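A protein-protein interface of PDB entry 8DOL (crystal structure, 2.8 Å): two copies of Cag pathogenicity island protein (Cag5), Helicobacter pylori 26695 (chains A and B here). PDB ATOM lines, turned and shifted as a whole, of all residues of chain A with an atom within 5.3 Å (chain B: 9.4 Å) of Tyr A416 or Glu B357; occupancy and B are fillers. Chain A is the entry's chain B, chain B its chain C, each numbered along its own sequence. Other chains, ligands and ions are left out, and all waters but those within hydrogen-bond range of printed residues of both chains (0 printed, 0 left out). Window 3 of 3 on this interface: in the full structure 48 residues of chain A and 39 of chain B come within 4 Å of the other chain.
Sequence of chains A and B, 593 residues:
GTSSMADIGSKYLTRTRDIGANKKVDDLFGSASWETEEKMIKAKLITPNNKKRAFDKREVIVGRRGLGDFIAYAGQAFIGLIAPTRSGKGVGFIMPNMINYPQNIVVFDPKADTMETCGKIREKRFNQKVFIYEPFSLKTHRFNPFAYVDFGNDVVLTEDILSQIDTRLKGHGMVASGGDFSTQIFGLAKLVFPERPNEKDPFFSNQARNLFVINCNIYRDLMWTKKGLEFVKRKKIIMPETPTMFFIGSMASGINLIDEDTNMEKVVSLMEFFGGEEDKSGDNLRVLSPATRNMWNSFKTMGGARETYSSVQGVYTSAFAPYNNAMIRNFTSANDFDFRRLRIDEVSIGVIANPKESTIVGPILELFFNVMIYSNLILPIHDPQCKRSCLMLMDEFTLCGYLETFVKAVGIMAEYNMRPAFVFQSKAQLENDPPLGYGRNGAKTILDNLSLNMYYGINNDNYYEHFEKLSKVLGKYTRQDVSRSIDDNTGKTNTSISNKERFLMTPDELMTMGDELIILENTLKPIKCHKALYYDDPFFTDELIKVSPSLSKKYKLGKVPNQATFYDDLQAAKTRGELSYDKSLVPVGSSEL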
ATOM      1  N   GLN A  76      13.867  -6.307  23.343  1.00  0.00           N
ATOM      2  CA  GLN A  76      14.806  -7.359  23.704  1.00  0.00           C
ATOM      3  C   GLN A  76      15.851  -6.923  24.722  1.00  0.00           C
ATOM      4  O   GLN A  76      16.731  -7.724  25.058  1.00  0.00           O
ATOM      5  CB  GLN A  76      15.516  -7.895  22.451  1.00  0.00           C
ATOM      6  CG  GLN A  76      14.614  -8.072  21.244  1.00  0.00           C
ATOM      7  CD  GLN A  76      15.391  -8.420  19.987  1.00  0.00           C
ATOM      8  OE1 GLN A  76      16.212  -7.635  19.513  1.00  0.00           O
ATOM      9  NE2 GLN A  76      15.135  -9.603  19.441  1.00  0.00           N
ATOM     10  N   ARG A 343      14.114 -22.261  22.185  1.00  0.00           N
ATOM     11  CA  ARG A 343      13.305 -21.237  21.539  1.00  0.00           C
ATOM     12  C   ARG A 343      12.300 -21.826  20.557  1.00  0.00           C
ATOM     13  O   ARG A 343      11.680 -21.080  19.791  1.00  0.00           O
ATOM     14  CB  ARG A 343      14.206 -20.225  20.828  1.00  0.00           C
ATOM     15  CG  ARG A 343      15.036 -19.376  21.769  1.00  0.00           C
ATOM     16  CD  ARG A 343      16.100 -18.605  21.012  1.00  0.00           C
ATOM     17  NE  ARG A 343      16.939 -19.479  20.204  1.00  0.00           N
ATOM     18  CZ  ARG A 343      17.533 -19.116  19.077  1.00  0.00           C
ATOM     19  NH1 ARG A 343      17.402 -17.893  18.588  1.00  0.00           N
ATOM     20  NH2 ARG A 343      18.281 -20.002  18.422  1.00  0.00           N
ATOM     21  N   TYR A 374      24.848 -21.195  24.417  1.00  0.00           N
ATOM     22  CA  TYR A 374      25.534 -21.409  23.153  1.00  0.00           C
ATOM     23  C   TYR A 374      24.822 -22.405  22.248  1.00  0.00           C
ATOM     24  O   TYR A 374      25.333 -22.714  21.167  1.00  0.00           O
ATOM     25  CB  TYR A 374      26.980 -21.845  23.411  1.00  0.00           C
ATOM     26  CG  TYR A 374      27.881 -20.668  23.714  1.00  0.00           C
ATOM     27  CD1 TYR A 374      28.344 -19.846  22.694  1.00  0.00           C
ATOM     28  CD2 TYR A 374      28.242 -20.358  25.018  1.00  0.00           C
ATOM     29  CE1 TYR A 374      29.156 -18.757  22.963  1.00  0.00           C
ATOM     30  CE2 TYR A 374      29.055 -19.272  25.297  1.00  0.00           C
ATOM     31  CZ  TYR A 374      29.508 -18.475  24.264  1.00  0.00           C
ATOM     32  OH  TYR A 374      30.317 -17.393  24.532  1.00  0.00           O
ATOM     33  N   ASN A 376      21.835 -21.524  21.194  1.00  0.00           N
ATOM     34  CA  ASN A 376      20.820 -20.637  20.638  1.00  0.00           C
ATOM     35  C   ASN A 376      21.443 -19.348  20.107  1.00  0.00           C
ATOM     36  O   ASN A 376      20.947 -18.247  20.349  1.00  0.00           O
ATOM     37  CB  ASN A 376      19.745 -20.321  21.678  1.00  0.00           C
ATOM     38  CG  ASN A 376      18.988 -21.557  22.137  1.00  0.00           C
ATOM     39  OD1 ASN A 376      17.946 -21.905  21.579  1.00  0.00           O
ATOM     40  ND2 ASN A 376      19.506 -22.221  23.164  1.00  0.00           N
ATOM     41  N   LEU A 377      22.544 -19.464  19.363  1.00  0.00           N
ATOM     42  CA  LEU A 377      23.028 -18.348  18.548  1.00  0.00           C
ATOM     43  C   LEU A 377      22.545 -18.464  17.114  1.00  0.00           C
ATOM     44  O   LEU A 377      23.279 -18.148  16.174  1.00  0.00           O
ATOM     45  CB  LEU A 377      24.549 -18.232  18.575  1.00  0.00           C
ATOM     46  CG  LEU A 377      25.275 -18.038  19.903  1.00  0.00           C
ATOM     47  CD1 LEU A 377      24.481 -17.132  20.851  1.00  0.00           C
ATOM     48  CD2 LEU A 377      25.605 -19.366  20.514  1.00  0.00           C
ATOM     49  N   ILE A 378      21.313 -18.920  16.924  1.00  0.00           N
ATOM     50  CA  ILE A 378      20.687 -18.992  15.612  1.00  0.00           C
ATOM     51  C   ILE A 378      19.587 -17.942  15.573  1.00  0.00           C
ATOM     52  O   ILE A 378      18.656 -17.980  16.386  1.00  0.00           O
ATOM     53  CB  ILE A 378      20.131 -20.392  15.320  1.00  0.00           C
ATOM     54  CG1 ILE A 378      21.004 -21.459  15.989  1.00  0.00           C
ATOM     55  CG2 ILE A 378      20.044 -20.626  13.821  1.00  0.00           C
ATOM     56  CD1 ILE A 378      22.344 -21.673  15.314  1.00  0.00           C
ATOM     57  N   LEU A 379      19.708 -16.995  14.647  1.00  0.00           N
ATOM     58  CA  LEU A 379      18.687 -15.975  14.487  1.00  0.00           C
ATOM     59  C   LEU A 379      17.383 -16.605  14.000  1.00  0.00           C
ATOM     60  O   LEU A 379      17.399 -17.564  13.223  1.00  0.00           O
ATOM     61  CB  LEU A 379      19.149 -14.910  13.499  1.00  0.00           C
ATOM     62  CG  LEU A 379      20.015 -13.770  14.028  1.00  0.00           C
ATOM     63  CD1 LEU A 379      20.038 -12.621  13.033  1.00  0.00           C
ATOM     64  CD2 LEU A 379      19.511 -13.297  15.374  1.00  0.00           C
ATOM     65  N   PRO A 380      16.237 -16.088  14.451  1.00  0.00           N
ATOM     66  CA  PRO A 380      14.953 -16.620  13.958  1.00  0.00           C
ATOM     67  C   PRO A 380      14.790 -16.504  12.452  1.00  0.00           C
ATOM     68  O   PRO A 380      13.989 -17.248  11.874  1.00  0.00           O
ATOM     69  CB  PRO A 380      13.895 -15.788  14.699  1.00  0.00           C
ATOM     70  CG  PRO A 380      14.611 -14.961  15.696  1.00  0.00           C
ATOM     71  CD  PRO A 380      16.085 -15.066  15.500  1.00  0.00           C
ATOM     72  N   ILE A 412      25.819 -10.258  23.148  1.00  0.00           N
ATOM     73  CA  ILE A 412      25.344 -10.794  21.876  1.00  0.00           C
ATOM     74  C   ILE A 412      24.086 -11.629  22.076  1.00  0.00           C
ATOM     75  O   ILE A 412      23.467 -12.074  21.103  1.00  0.00           O
ATOM     76  CB  ILE A 412      26.437 -11.630  21.183  1.00  0.00           C
ATOM     77  CG1 ILE A 412      27.021 -12.650  22.163  1.00  0.00           C
ATOM     78  CG2 ILE A 412      27.525 -10.729  20.613  1.00  0.00           C
ATOM     79  CD1 ILE A 412      27.460 -13.941  21.518  1.00  0.00           C
ATOM     80  N   MET A 413      23.708 -11.868  23.334  1.00  0.00           N
ATOM     81  CA  MET A 413      22.543 -12.711  23.595  1.00  0.00           C
ATOM     82  C   MET A 413      21.219 -12.051  23.216  1.00  0.00           C
ATOM     83  O   MET A 413      20.250 -12.765  22.941  1.00  0.00           O
ATOM     84  CB  MET A 413      22.495 -13.113  25.070  1.00  0.00           C
ATOM     85  CG  MET A 413      23.490 -14.182  25.453  1.00  0.00           C
ATOM     86  SD  MET A 413      23.187 -14.896  27.081  1.00  0.00           S
ATOM     87  CE  MET A 413      21.925 -13.813  27.727  1.00  0.00           C
ATOM     88  N   ALA A 414      21.159 -10.717  23.182  1.00  0.00           N
ATOM     89  CA  ALA A 414      19.872 -10.028  23.102  1.00  0.00           C
ATOM     90  C   ALA A 414      19.142 -10.338  21.799  1.00  0.00           C
ATOM     91  O   ALA A 414      17.936 -10.613  21.803  1.00  0.00           O
ATOM     92  CB  ALA A 414      20.076  -8.521  23.258  1.00  0.00           C
ATOM     93  N   GLU A 415      19.854 -10.297  20.671  1.00  0.00           N
ATOM     94  CA  GLU A 415      19.193 -10.446  19.380  1.00  0.00           C
ATOM     95  C   GLU A 415      18.665 -11.855  19.148  1.00  0.00           C
ATOM     96  O   GLU A 415      17.815 -12.048  18.272  1.00  0.00           O
ATOM     97  CB  GLU A 415      20.150 -10.051  18.254  1.00  0.00           C
ATOM     98  CG  GLU A 415      20.214  -8.552  18.002  1.00  0.00           C
ATOM     99  CD  GLU A 415      21.096  -7.825  19.003  1.00  0.00           C
ATOM    100  OE1 GLU A 415      21.781  -8.502  19.802  1.00  0.00           O
ATOM    101  OE2 GLU A 415      21.106  -6.576  18.991  1.00  0.00           O
ATOM    102  N   TYR A 416      19.138 -12.838  19.909  1.00  0.00           N
ATOM    103  CA  TYR A 416      18.649 -14.205  19.802  1.00  0.00           C
ATOM    104  C   TYR A 416      17.472 -14.482  20.728  1.00  0.00           C
ATOM    105  O   TYR A 416      17.115 -15.648  20.921  1.00  0.00           O
ATOM    106  CB  TYR A 416      19.780 -15.195  20.085  1.00  0.00           C
ATOM    107  CG  TYR A 416      20.954 -15.059  19.144  1.00  0.00           C
ATOM    108  CD1 TYR A 416      20.848 -15.443  17.815  1.00  0.00           C
ATOM    109  CD2 TYR A 416      22.169 -14.550  19.585  1.00  0.00           C
ATOM    110  CE1 TYR A 416      21.915 -15.317  16.949  1.00  0.00           C
ATOM    111  CE2 TYR A 416      23.244 -14.426  18.726  1.00  0.00           C
ATOM    112  CZ  TYR A 416      23.111 -14.812  17.409  1.00  0.00           C
ATOM    113  OH  TYR A 416      24.173 -14.693  16.542  1.00  0.00           O
ATOM    114  N   ASN A 417      16.866 -13.439  21.300  1.00  0.00           N
ATOM    115  CA  ASN A 417      15.698 -13.562  22.177  1.00  0.00           C
ATOM    116  C   ASN A 417      16.001 -14.384  23.425  1.00  0.00           C
ATOM    117  O   ASN A 417      15.109 -15.011  24.002  1.00  0.00           O
ATOM    118  CB  ASN A 417      14.495 -14.145  21.431  1.00  0.00           C
ATOM    119  CG  ASN A 417      14.123 -13.329  20.211  1.00  0.00           C
ATOM    120  OD1 ASN A 417      14.132 -12.098  20.249  1.00  0.00           O
ATOM    121  ND2 ASN A 417      13.800 -14.013  19.116  1.00  0.00           N
ATOM    122  N   MET A 418      17.259 -14.393  23.847  1.00  0.00           N
ATOM    123  CA  MET A 418      17.646 -14.911  25.156  1.00  0.00           C
ATOM    124  C   MET A 418      17.744 -13.698  26.076  1.00  0.00           C
ATOM    125  O   MET A 418      18.752 -12.988  26.077  1.00  0.00           O
ATOM    126  CB  MET A 418      18.963 -15.678  25.082  1.00  0.00           C
ATOM    127  CG  MET A 418      18.933 -16.955  24.242  1.00  0.00           C
ATOM    128  SD  MET A 418      18.078 -18.314  25.067  1.00  0.00           S
ATOM    129  CE  MET A 418      19.358 -19.562  25.076  1.00  0.00           C
ATOM    130  N   PRO B 110      29.652  -7.207  12.414  1.00  0.00           N
ATOM    131  CA  PRO B 110      29.415  -8.542  12.979  1.00  0.00           C
ATOM    132  C   PRO B 110      27.971  -8.997  12.826  1.00  0.00           C
ATOM    133  O   PRO B 110      27.699 -10.201  12.773  1.00  0.00           O
ATOM    134  CB  PRO B 110      29.795  -8.376  14.459  1.00  0.00           C
ATOM    135  CG  PRO B 110      30.302  -6.949  14.609  1.00  0.00           C
ATOM    136  CD  PRO B 110      29.751  -6.178  13.457  1.00  0.00           C
ATOM    137  N   LYS B 111      27.039  -8.049  12.753  1.00  0.00           N
ATOM    138  CA  LYS B 111      25.617  -8.364  12.691  1.00  0.00           C
ATOM    139  C   LYS B 111      25.074  -8.423  11.268  1.00  0.00           C
ATOM    140  O   LYS B 111      23.879  -8.679  11.089  1.00  0.00           O
ATOM    141  CB  LYS B 111      24.817  -7.344  13.510  1.00  0.00           C
ATOM    142  CG  LYS B 111      24.823  -7.620  15.007  1.00  0.00           C
ATOM    143  CD  LYS B 111      23.870  -6.699  15.752  1.00  0.00           C
ATOM    144  CE  LYS B 111      23.888  -6.980  17.249  1.00  0.00           C
ATOM    145  NZ  LYS B 111      24.657  -5.960  18.018  1.00  0.00           N
ATOM    146  N   ALA B 112      25.917  -8.185  10.261  1.00  0.00           N
ATOM    147  CA  ALA B 112      25.559  -8.303   8.848  1.00  0.00           C
ATOM    148  C   ALA B 112      24.460  -7.334   8.429  1.00  0.00           C
ATOM    149  O   ALA B 112      23.731  -7.598   7.467  1.00  0.00           O
ATOM    150  CB  ALA B 112      25.152  -9.740   8.497  1.00  0.00           C
ATOM    151  N   PHE B 136      32.976 -17.624   7.883  1.00  0.00           N
ATOM    152  CA  PHE B 136      32.049 -18.714   8.194  1.00  0.00           C
ATOM    153  C   PHE B 136      30.890 -18.790   7.215  1.00  0.00           C
ATOM    154  O   PHE B 136      29.737 -18.991   7.611  1.00  0.00           O
ATOM    155  CB  PHE B 136      31.545 -18.569   9.625  1.00  0.00           C
ATOM    156  CG  PHE B 136      32.522 -19.046  10.659  1.00  0.00           C
ATOM    157  CD1 PHE B 136      33.859 -19.230  10.339  1.00  0.00           C
ATOM    158  CD2 PHE B 136      32.105 -19.325  11.946  1.00  0.00           C
ATOM    159  CE1 PHE B 136      34.761 -19.671  11.286  1.00  0.00           C
ATOM    160  CE2 PHE B 136      33.000 -19.769  12.894  1.00  0.00           C
ATOM    161  CZ  PHE B 136      34.331 -19.941  12.566  1.00  0.00           C
ATOM    162  N   ILE B 352      32.897  -9.672   8.308  1.00  0.00           N
ATOM    163  CA  ILE B 352      31.864 -10.340   9.091  1.00  0.00           C
ATOM    164  C   ILE B 352      32.564 -11.341   9.998  1.00  0.00           C
ATOM    165  O   ILE B 352      33.165 -12.310   9.522  1.00  0.00           O
ATOM    166  CB  ILE B 352      30.835 -11.040   8.194  1.00  0.00           C
ATOM    167  CG1 ILE B 352      30.067 -10.021   7.345  1.00  0.00           C
ATOM    168  CG2 ILE B 352      29.887 -11.876   9.048  1.00  0.00           C
ATOM    169  CD1 ILE B 352      28.736  -9.611   7.917  1.00  0.00           C
ATOM    170  N   ALA B 353      32.488 -11.116  11.307  1.00  0.00           N
ATOM    171  CA  ALA B 353      33.115 -12.010  12.269  1.00  0.00           C
ATOM    172  C   ALA B 353      32.521 -11.744  13.642  1.00  0.00           C
ATOM    173  O   ALA B 353      32.206 -10.599  13.977  1.00  0.00           O
ATOM    174  CB  ALA B 353      34.637 -11.823  12.301  1.00  0.00           C
ATOM    175  N   ASN B 354      32.372 -12.809  14.426  1.00  0.00           N
ATOM    176  CA  ASN B 354      31.864 -12.731  15.795  1.00  0.00           C
ATOM    177  C   ASN B 354      32.767 -13.575  16.684  1.00  0.00           C
ATOM    178  O   ASN B 354      32.425 -14.714  17.033  1.00  0.00           O
ATOM    179  CB  ASN B 354      30.410 -13.196  15.873  1.00  0.00           C
ATOM    180  CG  ASN B 354      29.637 -12.508  16.980  1.00  0.00           C
ATOM    181  OD1 ASN B 354      30.180 -12.221  18.045  1.00  0.00           O
ATOM    182  ND2 ASN B 354      28.360 -12.242  16.732  1.00  0.00           N
ATOM    183  N   PRO B 355      33.937 -13.051  17.061  1.00  0.00           N
ATOM    184  CA  PRO B 355      34.845 -13.826  17.925  1.00  0.00           C
ATOM    185  C   PRO B 355      34.245 -14.204  19.268  1.00  0.00           C
ATOM    186  O   PRO B 355      34.685 -15.194  19.866  1.00  0.00           O
ATOM    187  CB  PRO B 355      36.052 -12.892  18.093  1.00  0.00           C
ATOM    188  CG  PRO B 355      36.012 -12.006  16.891  1.00  0.00           C
ATOM    189  CD  PRO B 355      34.556 -11.799  16.593  1.00  0.00           C
ATOM    190  N   LYS B 356      33.259 -13.452  19.766  1.00  0.00           N
ATOM    191  CA  LYS B 356      32.602 -13.835  21.012  1.00  0.00           C
ATOM    192  C   LYS B 356      31.809 -15.125  20.852  1.00  0.00           C
ATOM    193  O   LYS B 356      31.649 -15.876  21.821  1.00  0.00           O
ATOM    194  CB  LYS B 356      31.689 -12.709  21.503  1.00  0.00           C
ATOM    195  CG  LYS B 356      32.428 -11.479  22.007  1.00  0.00           C
ATOM    196  CD  LYS B 356      32.830 -11.630  23.463  1.00  0.00           C
ATOM    197  CE  LYS B 356      34.230 -11.087  23.702  1.00  0.00           C
ATOM    198  NZ  LYS B 356      35.284 -12.022  23.216  1.00  0.00           N
ATOM    199  N   GLU B 357      31.303 -15.396  19.649  1.00  0.00           N
ATOM    200  CA  GLU B 357      30.644 -16.670  19.384  1.00  0.00           C
ATOM    201  C   GLU B 357      31.669 -17.749  19.062  1.00  0.00           C
ATOM    202  O   GLU B 357      31.749 -18.775  19.747  1.00  0.00           O
ATOM    203  CB  GLU B 357      29.646 -16.521  18.232  1.00  0.00           C
ATOM    204  CG  GLU B 357      28.579 -15.469  18.461  1.00  0.00           C
ATOM    205  CD  GLU B 357      27.533 -15.453  17.363  1.00  0.00           C
ATOM    206  OE1 GLU B 357      27.586 -16.331  16.476  1.00  0.00           O
ATOM    207  OE2 GLU B 357      26.660 -14.559  17.391  1.00  0.00           O
ATOM    208  N   SER B 358      32.465 -17.529  18.020  1.00  0.00           N
ATOM    209  CA  SER B 358      33.510 -18.459  17.603  1.00  0.00           C
ATOM    210  C   SER B 358      34.844 -17.903  18.087  1.00  0.00           C
ATOM    211  O   SER B 358      35.424 -17.013  17.462  1.00  0.00           O
ATOM    212  CB  SER B 358      33.492 -18.644  16.091  1.00  0.00           C
ATOM    213  OG  SER B 358      32.166 -18.574  15.596  1.00  0.00           O
ATOM    214  N   THR B 359      35.330 -18.436  19.207  1.00  0.00           N
ATOM    215  CA  THR B 359      36.550 -17.941  19.830  1.00  0.00           C
ATOM    216  C   THR B 359      37.814 -18.335  19.079  1.00  0.00           C
ATOM    217  O   THR B 359      38.911 -17.991  19.532  1.00  0.00           O
ATOM    218  CB  THR B 359      36.635 -18.442  21.273  1.00  0.00           C
ATOM    219  OG1 THR B 359      37.966 -18.255  21.769  1.00  0.00           O
ATOM    220  CG2 THR B 359      36.275 -19.920  21.341  1.00  0.00           C
ATOM    221  N   ILE B 360      37.697 -19.038  17.947  1.00  0.00           N
ATOM    222  CA  ILE B 360      38.873 -19.502  17.215  1.00  0.00           C
ATOM    223  C   ILE B 360      39.399 -18.480  16.217  1.00  0.00           C
ATOM    224  O   ILE B 360      40.537 -18.623  15.743  1.00  0.00           O
ATOM    225  CB  ILE B 360      38.568 -20.827  16.489  1.00  0.00           C
ATOM    226  CG1 ILE B 360      38.118 -20.570  15.046  1.00  0.00           C
ATOM    227  CG2 ILE B 360      37.523 -21.621  17.263  1.00  0.00           C
ATOM    228  CD1 ILE B 360      37.178 -21.624  14.484  1.00  0.00           C
ATOM    229  N   VAL B 361      38.618 -17.444  15.888  1.00  0.00           N
ATOM    230  CA  VAL B 361      39.037 -16.466  14.886  1.00  0.00           C
ATOM    231  C   VAL B 361      39.915 -15.372  15.471  1.00  0.00           C
ATOM    232  O   VAL B 361      40.277 -14.430  14.755  1.00  0.00           O
ATOM    233  CB  VAL B 361      37.792 -15.863  14.203  1.00  0.00           C
ATOM    234  CG1 VAL B 361      38.141 -15.270  12.839  1.00  0.00           C
ATOM    235  CG2 VAL B 361      36.699 -16.914  14.067  1.00  0.00           C
ATOM    236  N   GLY B 362      40.280 -15.466  16.748  1.00  0.00           N
ATOM    237  CA  GLY B 362      41.086 -14.453  17.391  1.00  0.00           C
ATOM    238  C   GLY B 362      42.416 -14.226  16.697  1.00  0.00           C
ATOM    239  O   GLY B 362      42.660 -13.172  16.099  1.00  0.00           O
ATOM    240  N   LEU B 399      34.356  -6.387  20.700  1.00  0.00           N
ATOM    241  CA  LEU B 399      34.008  -7.713  20.200  1.00  0.00           C
ATOM    242  C   LEU B 399      35.200  -8.397  19.546  1.00  0.00           C
ATOM    243  O   LEU B 399      35.312  -9.627  19.595  1.00  0.00           O
ATOM    244  CB  LEU B 399      32.845  -7.600  19.214  1.00  0.00           C
ATOM    245  CG  LEU B 399      31.765  -8.682  19.159  1.00  0.00           C
ATOM    246  CD1 LEU B 399      30.677  -8.265  18.189  1.00  0.00           C
ATOM    247  CD2 LEU B 399      32.340 -10.019  18.747  1.00  0.00           C
ATOM    248  N   CYS B 400      36.106  -7.620  18.943  1.00  0.00           N
ATOM    249  CA  CYS B 400      37.236  -8.205  18.227  1.00  0.00           C
ATOM    250  C   CYS B 400      38.146  -9.002  19.154  1.00  0.00           C
ATOM    251  O   CYS B 400      38.837  -9.923  18.701  1.00  0.00           O
ATOM    252  CB  CYS B 400      38.029  -7.105  17.519  1.00  0.00           C
ATOM    253  SG  CYS B 400      37.486  -6.753  15.827  1.00  0.00           S
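O of Lys B356 is in hydrogen-bond range of OH of Tyr A374. The side-chain carboxylate (OE2) of Glu A415 lies within salt-bridge range of the side-chain amino group (NZ) of Lys B111 (3.7 Å). The side-chain hydroxyl (OH) of Tyr A416 lies within hydrogen-bond range of the side-chain carboxylate (OE2) of Glu B357.
The guanidinium group (NH1) of Arg A343 sits close to the backbone carbonyl oxygen (O) of Tyr A416. The side-chain carboxylate (OE2) of Glu B357 lies within hydrogen-bond range of the side-chain amide nitrogen (ND2) of Asn B354 (2.9 Å).
CG2 of Ile A412 touches OD1 of Asn B354 (3.98 Å). Glu B357 touches Ile A412.
Printed residues of chain B within 4 Å of Tyr A416: Glu B357 (2.6 Å). Glu B357 touches just these residues of chain A: Ile A412 (3.6 Å) and Tyr A416 (2.6 Å). No residue of chain B comes within 4 Å of Leu A377. Of the printed residues of chain A, Lys B111 touches Glu A415. Of the printed residues of chain B, Ile A412 touches Asn B354 (3.98 Å) and Glu B357 (3.6 Å). Printed residues of chain B within 4 Å of Glu A415: Lys B111 (3.3 Å). Of the printed residues of chain B, Tyr A374 touches Lys B356 (3.4 Å). Of the printed residues of chain A, Lys B356 touches Tyr A374. Val B361 touches none of the printed residues of chain A. The nearest residue of chain B that does not touch Tyr A416 is Asn B354 (4.9 Å). The nearest printed residue of chain A that does not touch Glu B357 is Tyr A374 (4.1 Å).
Of the 15 printed residues of chain A, 4 touch a printed residue of chain B. Hydrophobic or aromatic side chains of chain A that line the printed part of chain B: Tyr A374, Ile A412 and Tyr A416. Along chain B the printed residues that touch a printed residue of chain A span positions 111 to 357. Among the printed residues, 5 pairs touch across the chains. Among the printed residues, Asp or Glu carboxylates within 4 Å of a Lys or Arg side-chain nitrogen of the other chain: Glu A415 with Lys B111.
No position is printed for both chains. Of the 5 pairs that touch across the chains among the printed residues, none has its exchanged pair printed and touching as well.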
